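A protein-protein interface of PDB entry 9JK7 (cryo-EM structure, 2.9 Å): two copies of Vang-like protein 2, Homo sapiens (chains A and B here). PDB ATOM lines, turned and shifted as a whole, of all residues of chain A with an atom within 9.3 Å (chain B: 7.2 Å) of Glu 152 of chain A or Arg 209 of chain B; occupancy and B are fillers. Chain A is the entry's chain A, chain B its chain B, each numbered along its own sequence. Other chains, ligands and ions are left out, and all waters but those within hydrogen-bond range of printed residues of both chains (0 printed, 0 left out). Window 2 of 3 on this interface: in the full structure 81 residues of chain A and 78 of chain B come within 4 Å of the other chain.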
ATOM      1  N   LEU A 133      18.396 -22.590 -11.063  1.00  0.00           N
ATOM      2  CA  LEU A 133      18.173 -21.793  -9.865  1.00  0.00           C
ATOM      3  C   LEU A 133      17.035 -20.791 -10.012  1.00  0.00           C
ATOM      4  O   LEU A 133      16.504 -20.337  -8.994  1.00  0.00           O
ATOM      5  CB  LEU A 133      19.458 -21.061  -9.475  1.00  0.00           C
ATOM      6  CG  LEU A 133      20.607 -21.952  -9.004  1.00  0.00           C
ATOM      7  CD1 LEU A 133      21.873 -21.139  -8.788  1.00  0.00           C
ATOM      8  CD2 LEU A 133      20.221 -22.689  -7.735  1.00  0.00           C
ATOM      9  N   CYS A 147      13.839 -21.785   2.616  1.00  0.00           N
ATOM     10  CA  CYS A 147      15.044 -22.396   3.151  1.00  0.00           C
ATOM     11  C   CYS A 147      15.920 -21.335   3.801  1.00  0.00           C
ATOM     12  O   CYS A 147      15.781 -20.136   3.543  1.00  0.00           O
ATOM     13  CB  CYS A 147      15.821 -23.136   2.059  1.00  0.00           C
ATOM     14  SG  CYS A 147      16.419 -22.079   0.727  1.00  0.00           S
ATOM     15  N   GLY A 148      16.833 -21.796   4.652  1.00  0.00           N
ATOM     16  CA  GLY A 148      17.654 -20.905   5.447  1.00  0.00           C
ATOM     17  C   GLY A 148      18.837 -20.304   4.717  1.00  0.00           C
ATOM     18  O   GLY A 148      18.736 -19.930   3.545  1.00  0.00           O
ATOM     19  N   THR A 149      19.972 -20.209   5.412  1.00  0.00           N
ATOM     20  CA  THR A 149      21.147 -19.540   4.871  1.00  0.00           C
ATOM     21  C   THR A 149      22.016 -20.454   4.019  1.00  0.00           C
ATOM     22  O   THR A 149      22.857 -19.956   3.261  1.00  0.00           O
ATOM     23  CB  THR A 149      21.985 -18.962   6.009  1.00  0.00           C
ATOM     24  OG1 THR A 149      22.453 -20.028   6.844  1.00  0.00           O
ATOM     25  CG2 THR A 149      21.146 -18.011   6.844  1.00  0.00           C
ATOM     26  N   ALA A 150      21.848 -21.773   4.135  1.00  0.00           N
ATOM     27  CA  ALA A 150      22.620 -22.686   3.300  1.00  0.00           C
ATOM     28  C   ALA A 150      22.346 -22.435   1.824  1.00  0.00           C
ATOM     29  O   ALA A 150      23.259 -22.510   0.993  1.00  0.00           O
ATOM     30  CB  ALA A 150      22.304 -24.134   3.672  1.00  0.00           C
ATOM     31  N   CYS A 151      21.096 -22.112   1.483  1.00  0.00           N
ATOM     32  CA  CYS A 151      20.761 -21.786   0.103  1.00  0.00           C
ATOM     33  C   CYS A 151      21.580 -20.604  -0.397  1.00  0.00           C
ATOM     34  O   CYS A 151      22.157 -20.657  -1.484  1.00  0.00           O
ATOM     35  CB  CYS A 151      19.270 -21.489  -0.026  1.00  0.00           C
ATOM     36  SG  CYS A 151      18.198 -22.904   0.220  1.00  0.00           S
ATOM     37  N   GLU A 152      21.652 -19.529   0.391  1.00  0.00           N
ATOM     38  CA  GLU A 152      22.354 -18.334  -0.065  1.00  0.00           C
ATOM     39  C   GLU A 152      23.863 -18.551  -0.101  1.00  0.00           C
ATOM     40  O   GLU A 152      24.550 -18.034  -0.993  1.00  0.00           O
ATOM     41  CB  GLU A 152      21.995 -17.147   0.825  1.00  0.00           C
ATOM     42  CG  GLU A 152      20.545 -16.715   0.697  1.00  0.00           C
ATOM     43  CD  GLU A 152      20.203 -15.544   1.593  1.00  0.00           C
ATOM     44  OE1 GLU A 152      21.062 -15.147   2.408  1.00  0.00           O
ATOM     45  OE2 GLU A 152      19.075 -15.021   1.485  1.00  0.00           O
ATOM     46  N   GLY A 153      24.400 -19.306   0.858  1.00  0.00           N
ATOM     47  CA  GLY A 153      25.804 -19.675   0.777  1.00  0.00           C
ATOM     48  C   GLY A 153      26.112 -20.455  -0.485  1.00  0.00           C
ATOM     49  O   GLY A 153      27.130 -20.222  -1.146  1.00  0.00           O
ATOM     50  N   LEU A 154      25.219 -21.375  -0.856  1.00  0.00           N
ATOM     51  CA  LEU A 154      25.408 -22.105  -2.100  1.00  0.00           C
ATOM     52  C   LEU A 154      25.219 -21.207  -3.317  1.00  0.00           C
ATOM     53  O   LEU A 154      25.865 -21.430  -4.339  1.00  0.00           O
ATOM     54  CB  LEU A 154      24.464 -23.301  -2.158  1.00  0.00           C
ATOM     55  CG  LEU A 154      24.752 -24.424  -1.162  1.00  0.00           C
ATOM     56  CD1 LEU A 154      23.671 -25.487  -1.230  1.00  0.00           C
ATOM     57  CD2 LEU A 154      26.121 -25.030  -1.424  1.00  0.00           C
ATOM     58  N   PHE A 155      24.352 -20.193  -3.233  1.00  0.00           N
ATOM     59  CA  PHE A 155      24.264 -19.223  -4.325  1.00  0.00           C
ATOM     60  C   PHE A 155      25.587 -18.500  -4.518  1.00  0.00           C
ATOM     61  O   PHE A 155      26.032 -18.295  -5.652  1.00  0.00           O
ATOM     62  CB  PHE A 155      23.158 -18.193  -4.083  1.00  0.00           C
ATOM     63  CG  PHE A 155      21.769 -18.709  -4.303  1.00  0.00           C
ATOM     64  CD1 PHE A 155      21.324 -19.010  -5.577  1.00  0.00           C
ATOM     65  CD2 PHE A 155      20.874 -18.797  -3.255  1.00  0.00           C
ATOM     66  CE1 PHE A 155      20.039 -19.461  -5.788  1.00  0.00           C
ATOM     67  CE2 PHE A 155      19.591 -19.249  -3.456  1.00  0.00           C
ATOM     68  CZ  PHE A 155      19.171 -19.576  -4.725  1.00  0.00           C
ATOM     69  N   ILE A 156      26.227 -18.095  -3.421  1.00  0.00           N
ATOM     70  CA  ILE A 156      27.506 -17.398  -3.536  1.00  0.00           C
ATOM     71  C   ILE A 156      28.567 -18.332  -4.109  1.00  0.00           C
ATOM     72  O   ILE A 156      29.388 -17.933  -4.951  1.00  0.00           O
ATOM     73  CB  ILE A 156      27.931 -16.824  -2.173  1.00  0.00           C
ATOM     74  CG1 ILE A 156      26.854 -15.887  -1.638  1.00  0.00           C
ATOM     75  CG2 ILE A 156      29.223 -16.051  -2.311  1.00  0.00           C
ATOM     76  CD1 ILE A 156      27.071 -15.480  -0.206  1.00  0.00           C
ATOM     77  N   SER A 157      28.565 -19.592  -3.663  1.00  0.00           N
ATOM     78  CA  SER A 157      29.511 -20.561  -4.208  1.00  0.00           C
ATOM     79  C   SER A 157      29.272 -20.787  -5.696  1.00  0.00           C
ATOM     80  O   SER A 157      30.226 -20.883  -6.474  1.00  0.00           O
ATOM     81  CB  SER A 157      29.418 -21.881  -3.446  1.00  0.00           C
ATOM     82  OG  SER A 157      28.178 -22.518  -3.688  1.00  0.00           O
ATOM     83  N   VAL A 158      28.006 -20.868  -6.112  1.00  0.00           N
ATOM     84  CA  VAL A 158      27.685 -21.019  -7.529  1.00  0.00           C
ATOM     85  C   VAL A 158      28.155 -19.806  -8.312  1.00  0.00           C
ATOM     86  O   VAL A 158      28.681 -19.933  -9.419  1.00  0.00           O
ATOM     87  CB  VAL A 158      26.177 -21.262  -7.721  1.00  0.00           C
ATOM     88  CG1 VAL A 158      25.804 -21.164  -9.187  1.00  0.00           C
ATOM     89  CG2 VAL A 158      25.796 -22.625  -7.202  1.00  0.00           C
ATOM     90  N   ALA A 159      27.970 -18.611  -7.753  1.00  0.00           N
ATOM     91  CA  ALA A 159      28.418 -17.401  -8.433  1.00  0.00           C
ATOM     92  C   ALA A 159      29.918 -17.444  -8.684  1.00  0.00           C
ATOM     93  O   ALA A 159      30.380 -17.254  -9.817  1.00  0.00           O
ATOM     94  CB  ALA A 159      28.042 -16.169  -7.611  1.00  0.00           C
ATOM     95  N   PHE A 160      30.699 -17.723  -7.640  1.00  0.00           N
ATOM     96  CA  PHE A 160      32.148 -17.706  -7.814  1.00  0.00           C
ATOM     97  C   PHE A 160      32.634 -18.877  -8.662  1.00  0.00           C
ATOM     98  O   PHE A 160      33.607 -18.738  -9.408  1.00  0.00           O
ATOM     99  CB  PHE A 160      32.855 -17.675  -6.463  1.00  0.00           C
ATOM    100  CG  PHE A 160      32.846 -16.323  -5.823  1.00  0.00           C
ATOM    101  CD1 PHE A 160      33.747 -15.355  -6.230  1.00  0.00           C
ATOM    102  CD2 PHE A 160      31.934 -16.010  -4.834  1.00  0.00           C
ATOM    103  CE1 PHE A 160      33.743 -14.105  -5.658  1.00  0.00           C
ATOM    104  CE2 PHE A 160      31.927 -14.760  -4.259  1.00  0.00           C
ATOM    105  CZ  PHE A 160      32.834 -13.806  -4.670  1.00  0.00           C
ATOM    106  N   TYR A 218      13.707 -26.498  -2.032  1.00  0.00           N
ATOM    107  CA  TYR A 218      14.579 -25.691  -2.873  1.00  0.00           C
ATOM    108  C   TYR A 218      16.048 -25.939  -2.570  1.00  0.00           C
ATOM    109  O   TYR A 218      16.897 -25.697  -3.434  1.00  0.00           O
ATOM    110  CB  TYR A 218      14.227 -24.213  -2.703  1.00  0.00           C
ATOM    111  CG  TYR A 218      14.917 -23.277  -3.665  1.00  0.00           C
ATOM    112  CD1 TYR A 218      14.607 -23.292  -5.017  1.00  0.00           C
ATOM    113  CD2 TYR A 218      15.834 -22.338  -3.216  1.00  0.00           C
ATOM    114  CE1 TYR A 218      15.219 -22.430  -5.900  1.00  0.00           C
ATOM    115  CE2 TYR A 218      16.445 -21.465  -4.092  1.00  0.00           C
ATOM    116  CZ  TYR A 218      16.137 -21.519  -5.434  1.00  0.00           C
ATOM    117  OH  TYR A 218      16.743 -20.656  -6.315  1.00  0.00           O
ATOM    118  N   GLN A 219      16.362 -26.432  -1.369  1.00  0.00           N
ATOM    119  CA  GLN A 219      17.735 -26.813  -1.060  1.00  0.00           C
ATOM    120  C   GLN A 219      18.214 -27.924  -1.982  1.00  0.00           C
ATOM    121  O   GLN A 219      19.372 -27.929  -2.412  1.00  0.00           O
ATOM    122  CB  GLN A 219      17.848 -27.249   0.401  1.00  0.00           C
ATOM    123  CG  GLN A 219      17.610 -26.139   1.403  1.00  0.00           C
ATOM    124  CD  GLN A 219      17.719 -26.611   2.837  1.00  0.00           C
ATOM    125  OE1 GLN A 219      17.922 -27.796   3.101  1.00  0.00           O
ATOM    126  NE2 GLN A 219      17.580 -25.682   3.778  1.00  0.00           N
ATOM    127  N   VAL A 222      19.018 -26.349  -5.340  1.00  0.00           N
ATOM    128  CA  VAL A 222      20.253 -25.576  -5.268  1.00  0.00           C
ATOM    129  C   VAL A 222      21.461 -26.504  -5.232  1.00  0.00           C
ATOM    130  O   VAL A 222      22.471 -26.250  -5.895  1.00  0.00           O
ATOM    131  CB  VAL A 222      20.227 -24.627  -4.058  1.00  0.00           C
ATOM    132  CG1 VAL A 222      21.550 -23.918  -3.923  1.00  0.00           C
ATOM    133  CG2 VAL A 222      19.121 -23.616  -4.218  1.00  0.00           C
ATOM    134  N   VAL A 226      24.553 -26.808  -7.781  1.00  0.00           N
ATOM    135  CA  VAL A 226      25.936 -26.791  -7.304  1.00  0.00           C
ATOM    136  C   VAL A 226      26.704 -27.976  -7.872  1.00  0.00           C
ATOM    137  O   VAL A 226      27.856 -27.844  -8.304  1.00  0.00           O
ATOM    138  CB  VAL A 226      25.977 -26.785  -5.765  1.00  0.00           C
ATOM    139  CG1 VAL A 226      27.401 -26.952  -5.274  1.00  0.00           C
ATOM    140  CG2 VAL A 226      25.393 -25.503  -5.220  1.00  0.00           C
ATOM    141  N   TYR B 202      32.555 -14.409   1.418  1.00  0.00           N
ATOM    142  CA  TYR B 202      32.244 -15.492   2.341  1.00  0.00           C
ATOM    143  C   TYR B 202      32.232 -14.999   3.781  1.00  0.00           C
ATOM    144  O   TYR B 202      31.349 -15.373   4.555  1.00  0.00           O
ATOM    145  CB  TYR B 202      33.231 -16.641   2.155  1.00  0.00           C
ATOM    146  CG  TYR B 202      32.959 -17.459   0.923  1.00  0.00           C
ATOM    147  CD1 TYR B 202      31.716 -17.434   0.308  1.00  0.00           C
ATOM    148  CD2 TYR B 202      33.947 -18.240   0.356  1.00  0.00           C
ATOM    149  CE1 TYR B 202      31.471 -18.187  -0.823  1.00  0.00           C
ATOM    150  CE2 TYR B 202      33.703 -18.992  -0.772  1.00  0.00           C
ATOM    151  CZ  TYR B 202      32.469 -18.957  -1.357  1.00  0.00           C
ATOM    152  OH  TYR B 202      32.231 -19.706  -2.489  1.00  0.00           O
ATOM    153  N   TRP B 203      33.186 -14.142   4.156  1.00  0.00           N
ATOM    154  CA  TRP B 203      33.173 -13.594   5.508  1.00  0.00           C
ATOM    155  C   TRP B 203      31.963 -12.702   5.742  1.00  0.00           C
ATOM    156  O   TRP B 203      31.360 -12.748   6.816  1.00  0.00           O
ATOM    157  CB  TRP B 203      34.451 -12.814   5.800  1.00  0.00           C
ATOM    158  CG  TRP B 203      35.631 -13.655   6.140  1.00  0.00           C
ATOM    159  CD1 TRP B 203      36.709 -13.913   5.357  1.00  0.00           C
ATOM    160  CD2 TRP B 203      35.841 -14.369   7.362  1.00  0.00           C
ATOM    161  NE1 TRP B 203      37.592 -14.734   6.016  1.00  0.00           N
ATOM    162  CE2 TRP B 203      37.077 -15.029   7.251  1.00  0.00           C
ATOM    163  CE3 TRP B 203      35.105 -14.509   8.540  1.00  0.00           C
ATOM    164  CZ2 TRP B 203      37.593 -15.819   8.272  1.00  0.00           C
ATOM    165  CZ3 TRP B 203      35.617 -15.291   9.550  1.00  0.00           C
ATOM    166  CH2 TRP B 203      36.849 -15.936   9.411  1.00  0.00           C
ATOM    167  N   LEU B 204      31.608 -11.867   4.764  1.00  0.00           N
ATOM    168  CA  LEU B 204      30.436 -11.012   4.914  1.00  0.00           C
ATOM    169  C   LEU B 204      29.190 -11.843   5.159  1.00  0.00           C
ATOM    170  O   LEU B 204      28.446 -11.601   6.118  1.00  0.00           O
ATOM    171  CB  LEU B 204      30.254 -10.132   3.677  1.00  0.00           C
ATOM    172  CG  LEU B 204      31.266  -9.012   3.441  1.00  0.00           C
ATOM    173  CD1 LEU B 204      31.015  -8.353   2.094  1.00  0.00           C
ATOM    174  CD2 LEU B 204      31.208  -7.990   4.563  1.00  0.00           C
ATOM    175  N   PHE B 205      28.948 -12.836   4.301  1.00  0.00           N
ATOM    176  CA  PHE B 205      27.765 -13.671   4.467  1.00  0.00           C
ATOM    177  C   PHE B 205      27.812 -14.435   5.780  1.00  0.00           C
ATOM    178  O   PHE B 205      26.807 -14.525   6.495  1.00  0.00           O
ATOM    179  CB  PHE B 205      27.625 -14.638   3.297  1.00  0.00           C
ATOM    180  CG  PHE B 205      26.453 -15.552   3.428  1.00  0.00           C
ATOM    181  CD1 PHE B 205      25.173 -15.086   3.201  1.00  0.00           C
ATOM    182  CD2 PHE B 205      26.625 -16.871   3.804  1.00  0.00           C
ATOM    183  CE1 PHE B 205      24.089 -15.922   3.331  1.00  0.00           C
ATOM    184  CE2 PHE B 205      25.545 -17.712   3.934  1.00  0.00           C
ATOM    185  CZ  PHE B 205      24.275 -17.235   3.698  1.00  0.00           C
ATOM    186  N   TYR B 206      28.972 -15.000   6.112  1.00  0.00           N
ATOM    187  CA  TYR B 206      29.113 -15.757   7.348  1.00  0.00           C
ATOM    188  C   TYR B 206      28.786 -14.892   8.556  1.00  0.00           C
ATOM    189  O   TYR B 206      28.000 -15.289   9.422  1.00  0.00           O
ATOM    190  CB  TYR B 206      30.535 -16.307   7.440  1.00  0.00           C
ATOM    191  CG  TYR B 206      30.799 -17.151   8.652  1.00  0.00           C
ATOM    192  CD1 TYR B 206      30.367 -18.466   8.712  1.00  0.00           C
ATOM    193  CD2 TYR B 206      31.479 -16.631   9.741  1.00  0.00           C
ATOM    194  CE1 TYR B 206      30.612 -19.241   9.822  1.00  0.00           C
ATOM    195  CE2 TYR B 206      31.725 -17.396  10.854  1.00  0.00           C
ATOM    196  CZ  TYR B 206      31.288 -18.698  10.888  1.00  0.00           C
ATOM    197  OH  TYR B 206      31.537 -19.458  11.998  1.00  0.00           O
ATOM    198  N   GLY B 207      29.355 -13.693   8.614  1.00  0.00           N
ATOM    199  CA  GLY B 207      29.072 -12.766   9.685  1.00  0.00           C
ATOM    200  C   GLY B 207      27.613 -12.383   9.773  1.00  0.00           C
ATOM    201  O   GLY B 207      27.024 -12.447  10.855  1.00  0.00           O
ATOM    202  N   VAL B 208      27.005 -11.999   8.648  1.00  0.00           N
ATOM    203  CA  VAL B 208      25.668 -11.418   8.702  1.00  0.00           C
ATOM    204  C   VAL B 208      24.559 -12.451   8.820  1.00  0.00           C
ATOM    205  O   VAL B 208      23.469 -12.109   9.295  1.00  0.00           O
ATOM    206  CB  VAL B 208      25.397 -10.527   7.472  1.00  0.00           C
ATOM    207  CG1 VAL B 208      26.427  -9.412   7.387  1.00  0.00           C
ATOM    208  CG2 VAL B 208      25.366 -11.351   6.197  1.00  0.00           C
ATOM    209  N   ARG B 209      24.790 -13.701   8.415  1.00  0.00           N
ATOM    210  CA  ARG B 209      23.729 -14.698   8.409  1.00  0.00           C
ATOM    211  C   ARG B 209      24.042 -15.947   9.217  1.00  0.00           C
ATOM    212  O   ARG B 209      23.162 -16.804   9.356  1.00  0.00           O
ATOM    213  CB  ARG B 209      23.397 -15.107   6.966  1.00  0.00           C
ATOM    214  CG  ARG B 209      22.893 -13.958   6.111  1.00  0.00           C
ATOM    215  CD  ARG B 209      21.544 -13.461   6.597  1.00  0.00           C
ATOM    216  NE  ARG B 209      20.519 -14.491   6.495  1.00  0.00           N
ATOM    217  CZ  ARG B 209      19.794 -14.709   5.405  1.00  0.00           C
ATOM    218  NH1 ARG B 209      19.984 -13.962   4.326  1.00  0.00           N
ATOM    219  NH2 ARG B 209      18.878 -15.669   5.392  1.00  0.00           N
ATOM    220  N   ILE B 210      25.254 -16.082   9.749  1.00  0.00           N
ATOM    221  CA  ILE B 210      25.629 -17.239  10.549  1.00  0.00           C
ATOM    222  C   ILE B 210      26.170 -16.763  11.889  1.00  0.00           C
ATOM    223  O   ILE B 210      25.721 -17.208  12.949  1.00  0.00           O
ATOM    224  CB  ILE B 210      26.663 -18.109   9.815  1.00  0.00           C
ATOM    225  CG1 ILE B 210      26.041 -18.739   8.566  1.00  0.00           C
ATOM    226  CG2 ILE B 210      27.226 -19.158  10.748  1.00  0.00           C
ATOM    227  CD1 ILE B 210      27.043 -19.384   7.638  1.00  0.00           C
ATOM    228  N   LEU B 211      27.144 -15.853  11.846  1.00  0.00           N
ATOM    229  CA  LEU B 211      27.758 -15.365  13.076  1.00  0.00           C
ATOM    230  C   LEU B 211      26.807 -14.455  13.844  1.00  0.00           C
ATOM    231  O   LEU B 211      26.609 -14.625  15.052  1.00  0.00           O
ATOM    232  CB  LEU B 211      29.062 -14.637  12.757  1.00  0.00           C
ATOM    233  CG  LEU B 211      29.866 -14.128  13.952  1.00  0.00           C
ATOM    234  CD1 LEU B 211      30.347 -15.292  14.794  1.00  0.00           C
ATOM    235  CD2 LEU B 211      31.034 -13.276  13.489  1.00  0.00           C
ATOM    236  N   ASP B 212      26.209 -13.477  13.159  1.00  0.00           N
ATOM    237  CA  ASP B 212      25.292 -12.565  13.835  1.00  0.00           C
ATOM    238  C   ASP B 212      24.011 -13.279  14.242  1.00  0.00           C
ATOM    239  O   ASP B 212      23.558 -13.149  15.385  1.00  0.00           O
ATOM    240  CB  ASP B 212      24.977 -11.371  12.933  1.00  0.00           C
ATOM    241  CG  ASP B 212      24.255 -10.255  13.665  1.00  0.00           C
ATOM    242  OD1 ASP B 212      23.995 -10.395  14.878  1.00  0.00           O
ATOM    243  OD2 ASP B 212      23.942  -9.233  13.018  1.00  0.00           O
ATOM    244  N   ALA B 213      23.417 -14.042  13.325  1.00  0.00           N
ATOM    245  CA  ALA B 213      22.200 -14.782  13.630  1.00  0.00           C
ATOM    246  C   ALA B 213      22.444 -15.978  14.540  1.00  0.00           C
ATOM    247  O   ALA B 213      21.474 -16.627  14.945  1.00  0.00           O
ATOM    248  CB  ALA B 213      21.532 -15.252  12.336  1.00  0.00           C
ATOM    249  N   ARG B 214      23.702 -16.273  14.872  1.00  0.00           N
ATOM    250  CA  ARG B 214      24.068 -17.418  15.703  1.00  0.00           C
ATOM    251  C   ARG B 214      23.422 -18.695  15.168  1.00  0.00           C
ATOM    252  O   ARG B 214      22.595 -19.332  15.821  1.00  0.00           O
ATOM    253  CB  ARG B 214      23.692 -17.175  17.166  1.00  0.00           C
ATOM    254  CG  ARG B 214      24.488 -16.063  17.826  1.00  0.00           C
ATOM    255  CD  ARG B 214      24.087 -15.884  19.280  1.00  0.00           C
ATOM    256  NE  ARG B 214      24.756 -14.740  19.892  1.00  0.00           N
ATOM    257  CZ  ARG B 214      25.933 -14.801  20.506  1.00  0.00           C
ATOM    258  NH1 ARG B 214      26.579 -15.955  20.595  1.00  0.00           N
ATOM    259  NH2 ARG B 214      26.463 -13.706  21.035  1.00  0.00           N
ATOM    260  N   GLU B 215      23.818 -19.049  13.943  1.00  0.00           N
ATOM    261  CA  GLU B 215      23.181 -20.131  13.202  1.00  0.00           C
ATOM    262  C   GLU B 215      23.192 -21.432  13.993  1.00  0.00           C
ATOM    263  O   GLU B 215      24.258 -21.986  14.285  1.00  0.00           O
ATOM    264  CB  GLU B 215      23.868 -20.328  11.850  1.00  0.00           C
ATOM    265  CG  GLU B 215      23.215 -21.382  10.974  1.00  0.00           C
ATOM    266  CD  GLU B 215      21.821 -20.986  10.527  1.00  0.00           C
ATOM    267  OE1 GLU B 215      21.542 -19.773  10.437  1.00  0.00           O
ATOM    268  OE2 GLU B 215      20.999 -21.892  10.266  1.00  0.00           O
ATOM    269  N   VAL B 221      26.600 -24.552   8.274  1.00  0.00           N
ATOM    270  CA  VAL B 221      27.903 -23.906   8.395  1.00  0.00           C
ATOM    271  C   VAL B 221      28.995 -24.805   7.834  1.00  0.00           C
ATOM    272  O   VAL B 221      29.914 -24.342   7.145  1.00  0.00           O
ATOM    273  CB  VAL B 221      28.176 -23.539   9.865  1.00  0.00           C
ATOM    274  CG1 VAL B 221      29.529 -22.857  10.004  1.00  0.00           C
ATOM    275  CG2 VAL B 221      27.058 -22.673  10.410  1.00  0.00           C
ATOM    276  N   PHE B 224      28.839 -24.721   4.155  1.00  0.00           N
ATOM    277  CA  PHE B 224      29.373 -23.445   3.693  1.00  0.00           C
ATOM    278  C   PHE B 224      30.895 -23.472   3.663  1.00  0.00           C
ATOM    279  O   PHE B 224      31.518 -23.005   2.701  1.00  0.00           O
ATOM    280  CB  PHE B 224      28.851 -22.326   4.597  1.00  0.00           C
ATOM    281  CG  PHE B 224      29.240 -20.947   4.158  1.00  0.00           C
ATOM    282  CD1 PHE B 224      28.656 -20.371   3.044  1.00  0.00           C
ATOM    283  CD2 PHE B 224      30.155 -20.208   4.884  1.00  0.00           C
ATOM    284  CE1 PHE B 224      29.002 -19.097   2.644  1.00  0.00           C
ATOM    285  CE2 PHE B 224      30.501 -18.933   4.490  1.00  0.00           C
ATOM    286  CZ  PHE B 224      29.924 -18.378   3.369  1.00  0.00           C
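The backbone carbonyl oxygen (O) of Leu 154 of chain A is in hydrogen-bond range of the side-chain hydroxyl (OG) of Ser 157 of chain A (2.6 Å).
The backbone carbonyl oxygen of Ile 210 of chain B sits at hydrogen-bond distance from the backbone NH of Glu 215 of chain B, at 2.8 Å.
The side-chain sulfur (SG) of Cys 147 of chain A is disulfide-bonded to the side-chain sulfur (SG) of Cys 151 of chain A, at 2.0 Å.
Glu 152 of chain A touches two residues of chain B.
Of the printed residues of chain A, Tyr 202 of chain B touches Ile 156 (3.4 Å) and Ser 157 (3.3 Å).
No residue of chain A comes within 4 Å of Gly 207 of chain B.
No residue of chain A comes within 4 Å of Ile 210 of chain B.
Of the printed residues of chain A, Phe 224 of chain B touches Gly 153.
Printed residues of chain A that touch a printed residue of chain B: Thr 149, Glu 152, Gly 153, Ile 156 and Ser 157.
Hydrophobic or aromatic side chains of chain A that line the printed part of chain B: Ile 156.
Along chain A the printed residues that touch a printed residue of chain B span positions 149 to 157.
Hydrophobic or aromatic side chains of chain B within 4 Å of the printed part of chain A: Tyr 202, Phe 205 and Phe 224.
Among the printed residues, 10 pairs touch across the chains.
Among the printed residues, Asp or Glu carboxylates within 4 Å of a Lys or Arg side-chain nitrogen of the other chain: Glu 152 of chain A with Arg 209 of chain B (2.5 Å).
The side-chain carboxylate (OE1) of Glu 152 of chain A lies within salt-bridge range of the guanidinium group (NH1) of Arg 209 of chain B (2.5 Å).
No position is printed for both chains.
Among the printed residues, pairs that only touch across the chains: Thr 149 of chain A with Phe 205 of chain B (3.1 Å), Glu 152 of chain A with Phe 205 of chain B (3.3 Å), Ser 157 of chain A with Tyr 202 of chain B (3.3 Å), Ile 156 of chain A with Tyr 202 of chain B (3.4 Å), Thr 149 of chain A with Arg 209 of chain B (3.4 Å), Gly 153 of chain A with Phe 205 of chain B (3.5 Å), Ile 156 of chain A with Phe 205 of chain B (3.6 Å), Gly 153 of chain A with Phe 224 of chain B (3.7 Å) and Thr 149 of chain A with Glu 215 of chain B (3.7 Å).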
